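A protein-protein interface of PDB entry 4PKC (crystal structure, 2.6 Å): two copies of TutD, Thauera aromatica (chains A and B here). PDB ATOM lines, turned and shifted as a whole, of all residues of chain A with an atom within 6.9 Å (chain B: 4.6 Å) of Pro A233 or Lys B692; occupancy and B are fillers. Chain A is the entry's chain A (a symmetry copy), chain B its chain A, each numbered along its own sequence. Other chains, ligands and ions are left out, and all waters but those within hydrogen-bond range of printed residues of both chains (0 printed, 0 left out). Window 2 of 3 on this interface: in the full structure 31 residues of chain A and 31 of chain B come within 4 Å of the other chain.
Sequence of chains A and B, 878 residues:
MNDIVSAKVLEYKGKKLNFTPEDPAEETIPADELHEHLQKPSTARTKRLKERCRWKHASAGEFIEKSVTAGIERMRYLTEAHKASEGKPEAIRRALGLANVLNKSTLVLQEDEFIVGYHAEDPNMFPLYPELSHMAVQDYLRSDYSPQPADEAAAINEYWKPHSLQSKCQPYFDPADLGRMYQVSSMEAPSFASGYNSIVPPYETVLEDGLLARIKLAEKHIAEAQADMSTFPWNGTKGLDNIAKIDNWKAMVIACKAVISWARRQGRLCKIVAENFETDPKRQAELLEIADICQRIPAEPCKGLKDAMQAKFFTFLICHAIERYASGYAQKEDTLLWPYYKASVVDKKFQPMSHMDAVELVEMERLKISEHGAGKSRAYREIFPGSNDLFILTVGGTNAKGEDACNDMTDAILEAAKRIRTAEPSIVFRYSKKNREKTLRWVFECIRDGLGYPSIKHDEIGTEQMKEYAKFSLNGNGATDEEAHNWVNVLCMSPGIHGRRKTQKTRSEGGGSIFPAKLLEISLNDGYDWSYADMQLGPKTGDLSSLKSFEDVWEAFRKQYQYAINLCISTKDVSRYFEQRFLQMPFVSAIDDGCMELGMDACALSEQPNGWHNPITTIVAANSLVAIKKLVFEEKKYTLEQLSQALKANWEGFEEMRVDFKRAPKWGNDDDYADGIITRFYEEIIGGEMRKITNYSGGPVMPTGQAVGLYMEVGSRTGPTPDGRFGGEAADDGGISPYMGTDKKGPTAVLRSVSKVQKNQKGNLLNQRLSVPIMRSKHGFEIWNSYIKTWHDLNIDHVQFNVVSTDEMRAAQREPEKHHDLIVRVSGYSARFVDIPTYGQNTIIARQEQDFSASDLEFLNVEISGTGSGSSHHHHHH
N of Thr B694 is in hydrogen-bond range of O of Trp A234, at 3.1 Å. The side-chain amide nitrogen (ND2) of Asn B566 sits close to the backbone NH (N) of Trp A234.
The side-chain amino group (NZ) of Lys B692 lies within salt-bridge range of the side-chain carboxylate (OE1) of Glu B689 (2.7 Å).
Of chain B, only Asn B566 and Lys B692 come within 4 Å of Pro A233. Printed residues of chain A within 4 Å of Lys B692: Pro A233. Of the printed residues of chain B, Trp A234 touches Asn B566 (3.0 Å), Ile B693 (3.3 Å) and Thr B694 (3.1 Å). Of the printed residues of chain B, Phe A232 touches Asn B566 (3.3 Å) and Glu B689 (3.2 Å). Printed residues of chain B within 4 Å of Asn A235: Thr B694. Met B690 touches none of the printed residues of chain A. Asp A228 touches none of the printed residues of chain B. The nearest residue of chain A that does not touch Lys B692 is Phe A232 (4.1 Å).
Among the printed residues, merely in contact across the chains: Thr A231 with Asn B566, Phe A232 with Asn B566, Phe A232 with Glu B689, Pro A233 with Asn B566, Pro A233 with Lys B692, Trp A234 with Ile B693 and Asn A235 with Thr B694.
No position is printed for both chains.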
ATOM      1  N   ASP A 228      -0.993 -13.208  17.280  1.00  0.00           N
ATOM      2  CA  ASP A 228       0.031 -12.807  18.237  1.00  0.00           C
ATOM      3  C   ASP A 228       0.234 -13.863  19.319  1.00  0.00           C
ATOM      4  O   ASP A 228       1.359 -14.101  19.759  1.00  0.00           O
ATOM      5  CB  ASP A 228      -0.331 -11.468  18.883  1.00  0.00           C
ATOM      6  CG  ASP A 228       0.747 -10.969  19.826  1.00  0.00           C
ATOM      7  OD1 ASP A 228       1.924 -10.920  19.410  1.00  0.00           O
ATOM      8  OD2 ASP A 228       0.422 -10.638  20.985  1.00  0.00           O
ATOM      9  N   THR A 231       2.377 -16.618  18.151  1.00  0.00           N
ATOM     10  CA  THR A 231       3.627 -16.129  17.582  1.00  0.00           C
ATOM     11  C   THR A 231       4.824 -16.501  18.450  1.00  0.00           C
ATOM     12  O   THR A 231       4.897 -16.128  19.621  1.00  0.00           O
ATOM     13  CB  THR A 231       3.604 -14.600  17.390  1.00  0.00           C
ATOM     14  OG1 THR A 231       2.599 -14.251  16.432  1.00  0.00           O
ATOM     15  CG2 THR A 231       4.955 -14.104  16.900  1.00  0.00           C
ATOM     16  N   PHE A 232       5.760 -17.241  17.865  1.00  0.00           N
ATOM     17  CA  PHE A 232       6.993 -17.608  18.550  1.00  0.00           C
ATOM     18  C   PHE A 232       7.975 -16.441  18.518  1.00  0.00           C
ATOM     19  O   PHE A 232       8.150 -15.805  17.480  1.00  0.00           O
ATOM     20  CB  PHE A 232       7.611 -18.854  17.904  1.00  0.00           C
ATOM     21  CG  PHE A 232       8.869 -19.328  18.576  1.00  0.00           C
ATOM     22  CD1 PHE A 232       8.811 -20.202  19.649  1.00  0.00           C
ATOM     23  CD2 PHE A 232      10.112 -18.906  18.129  1.00  0.00           C
ATOM     24  CE1 PHE A 232       9.968 -20.640  20.267  1.00  0.00           C
ATOM     25  CE2 PHE A 232      11.270 -19.339  18.742  1.00  0.00           C
ATOM     26  CZ  PHE A 232      11.199 -20.209  19.812  1.00  0.00           C
ATOM     27  N   PRO A 233       8.626 -16.156  19.657  1.00  0.00           N
ATOM     28  CA  PRO A 233       8.469 -16.865  20.932  1.00  0.00           C
ATOM     29  C   PRO A 233       7.363 -16.285  21.809  1.00  0.00           C
ATOM     30  O   PRO A 233       7.095 -15.086  21.761  1.00  0.00           O
ATOM     31  CB  PRO A 233       9.835 -16.681  21.590  1.00  0.00           C
ATOM     32  CG  PRO A 233      10.275 -15.338  21.114  1.00  0.00           C
ATOM     33  CD  PRO A 233       9.717 -15.166  19.718  1.00  0.00           C
ATOM     34  N   TRP A 234       6.736 -17.140  22.611  1.00  0.00           N
ATOM     35  CA  TRP A 234       5.667 -16.720  23.509  1.00  0.00           C
ATOM     36  C   TRP A 234       6.214 -15.938  24.701  1.00  0.00           C
ATOM     37  O   TRP A 234       7.295 -16.231  25.208  1.00  0.00           O
ATOM     38  CB  TRP A 234       4.874 -17.942  23.989  1.00  0.00           C
ATOM     39  CG  TRP A 234       3.940 -17.663  25.129  1.00  0.00           C
ATOM     40  CD1 TRP A 234       4.202 -17.823  26.460  1.00  0.00           C
ATOM     41  CD2 TRP A 234       2.592 -17.184  25.041  1.00  0.00           C
ATOM     42  NE1 TRP A 234       3.103 -17.470  27.203  1.00  0.00           N
ATOM     43  CE2 TRP A 234       2.101 -17.074  26.358  1.00  0.00           C
ATOM     44  CE3 TRP A 234       1.753 -16.835  23.977  1.00  0.00           C
ATOM     45  CZ2 TRP A 234       0.811 -16.630  26.639  1.00  0.00           C
ATOM     46  CZ3 TRP A 234       0.471 -16.395  24.260  1.00  0.00           C
ATOM     47  CH2 TRP A 234       0.013 -16.296  25.580  1.00  0.00           C
ATOM     48  N   ASN A 235       5.460 -14.933  25.134  1.00  0.00           N
ATOM     49  CA  ASN A 235       5.822 -14.142  26.305  1.00  0.00           C
ATOM     50  C   ASN A 235       4.634 -14.030  27.252  1.00  0.00           C
ATOM     51  O   ASN A 235       3.716 -13.240  27.023  1.00  0.00           O
ATOM     52  CB  ASN A 235       6.306 -12.751  25.885  1.00  0.00           C
ATOM     53  CG  ASN A 235       7.023 -12.013  27.005  1.00  0.00           C
ATOM     54  OD1 ASN A 235       6.736 -12.212  28.186  1.00  0.00           O
ATOM     55  ND2 ASN A 235       7.960 -11.150  26.634  1.00  0.00           N
ATOM     56  N   ASN B 566       6.014 -23.738  21.806  1.00  0.00           N
ATOM     57  CA  ASN B 566       5.216 -22.532  21.975  1.00  0.00           C
ATOM     58  C   ASN B 566       3.837 -22.874  22.523  1.00  0.00           C
ATOM     59  O   ASN B 566       3.326 -22.193  23.410  1.00  0.00           O
ATOM     60  CB  ASN B 566       5.092 -21.777  20.651  1.00  0.00           C
ATOM     61  CG  ASN B 566       4.816 -20.299  20.848  1.00  0.00           C
ATOM     62  OD1 ASN B 566       3.665 -19.859  20.820  1.00  0.00           O
ATOM     63  ND2 ASN B 566       5.874 -19.523  21.055  1.00  0.00           N
ATOM     64  N   GLY B 688      18.235 -23.409  23.351  1.00  0.00           N
ATOM     65  CA  GLY B 688      18.279 -22.047  22.853  1.00  0.00           C
ATOM     66  C   GLY B 688      16.912 -21.484  22.519  1.00  0.00           C
ATOM     67  O   GLY B 688      16.505 -20.457  23.065  1.00  0.00           O
ATOM     68  N   GLU B 689      16.202 -22.158  21.619  1.00  0.00           N
ATOM     69  CA  GLU B 689      14.875 -21.723  21.194  1.00  0.00           C
ATOM     70  C   GLU B 689      13.886 -21.737  22.353  1.00  0.00           C
ATOM     71  O   GLU B 689      12.920 -20.974  22.372  1.00  0.00           O
ATOM     72  CB  GLU B 689      14.360 -22.611  20.060  1.00  0.00           C
ATOM     73  CG  GLU B 689      15.292 -22.705  18.863  1.00  0.00           C
ATOM     74  CD  GLU B 689      15.375 -21.410  18.080  1.00  0.00           C
ATOM     75  OE1 GLU B 689      14.472 -20.560  18.232  1.00  0.00           O
ATOM     76  OE2 GLU B 689      16.344 -21.243  17.311  1.00  0.00           O
ATOM     77  N   MET B 690      14.139 -22.612  23.319  1.00  0.00           N
ATOM     78  CA  MET B 690      13.259 -22.779  24.465  1.00  0.00           C
ATOM     79  C   MET B 690      13.458 -21.670  25.498  1.00  0.00           C
ATOM     80  O   MET B 690      12.515 -21.269  26.180  1.00  0.00           O
ATOM     81  CB  MET B 690      13.494 -24.150  25.099  1.00  0.00           C
ATOM     82  CG  MET B 690      12.636 -24.445  26.308  1.00  0.00           C
ATOM     83  SD  MET B 690      12.935 -26.109  26.927  1.00  0.00           S
ATOM     84  CE  MET B 690      12.148 -26.001  28.523  1.00  0.00           C
ATOM     85  N   ARG B 691      14.687 -21.176  25.603  1.00  0.00           N
ATOM     86  CA  ARG B 691      15.006 -20.092  26.528  1.00  0.00           C
ATOM     87  C   ARG B 691      14.381 -18.773  26.070  1.00  0.00           C
ATOM     88  O   ARG B 691      14.135 -17.875  26.877  1.00  0.00           O
ATOM     89  CB  ARG B 691      16.526 -19.943  26.671  1.00  0.00           C
ATOM     90  CG  ARG B 691      16.971 -18.826  27.606  1.00  0.00           C
ATOM     91  CD  ARG B 691      18.485 -18.684  27.632  1.00  0.00           C
ATOM     92  NE  ARG B 691      19.121 -19.697  28.468  1.00  0.00           N
ATOM     93  CZ  ARG B 691      19.473 -19.505  29.735  1.00  0.00           C
ATOM     94  NH1 ARG B 691      19.252 -18.331  30.314  1.00  0.00           N
ATOM     95  NH2 ARG B 691      20.048 -20.480  30.423  1.00  0.00           N
ATOM     96  N   LYS B 692      14.112 -18.671  24.771  1.00  0.00           N
ATOM     97  CA  LYS B 692      13.522 -17.467  24.190  1.00  0.00           C
ATOM     98  C   LYS B 692      12.117 -17.190  24.723  1.00  0.00           C
ATOM     99  O   LYS B 692      11.634 -16.059  24.669  1.00  0.00           O
ATOM    100  CB  LYS B 692      13.476 -17.580  22.665  1.00  0.00           C
ATOM    101  CG  LYS B 692      14.832 -17.774  22.010  1.00  0.00           C
ATOM    102  CD  LYS B 692      14.693 -17.897  20.503  1.00  0.00           C
ATOM    103  CE  LYS B 692      16.038 -18.128  19.838  1.00  0.00           C
ATOM    104  NZ  LYS B 692      15.900 -18.239  18.360  1.00  0.00           N
ATOM    105  N   ILE B 693      11.464 -18.229  25.234  1.00  0.00           N
ATOM    106  CA  ILE B 693      10.108 -18.104  25.755  1.00  0.00           C
ATOM    107  C   ILE B 693      10.101 -17.648  27.212  1.00  0.00           C
ATOM    108  O   ILE B 693      10.808 -18.207  28.051  1.00  0.00           O
ATOM    109  CB  ILE B 693       9.339 -19.438  25.642  1.00  0.00           C
ATOM    110  CG1 ILE B 693       9.317 -19.921  24.190  1.00  0.00           C
ATOM    111  CG2 ILE B 693       7.923 -19.290  26.176  1.00  0.00           C
ATOM    112  CD1 ILE B 693       8.535 -21.195  23.984  1.00  0.00           C
ATOM    113  N   THR B 694       9.303 -16.625  27.500  1.00  0.00           N
ATOM    114  CA  THR B 694       9.123 -16.143  28.865  1.00  0.00           C
ATOM    115  C   THR B 694       7.740 -16.540  29.369  1.00  0.00           C
ATOM    116  O   THR B 694       6.745 -16.348  28.673  1.00  0.00           O
ATOM    117  CB  THR B 694       9.285 -14.613  28.957  1.00  0.00           C
ATOM    118  OG1 THR B 694      10.534 -14.224  28.370  1.00  0.00           O
ATOM    119  CG2 THR B 694       9.242 -14.154  30.408  1.00  0.00           C
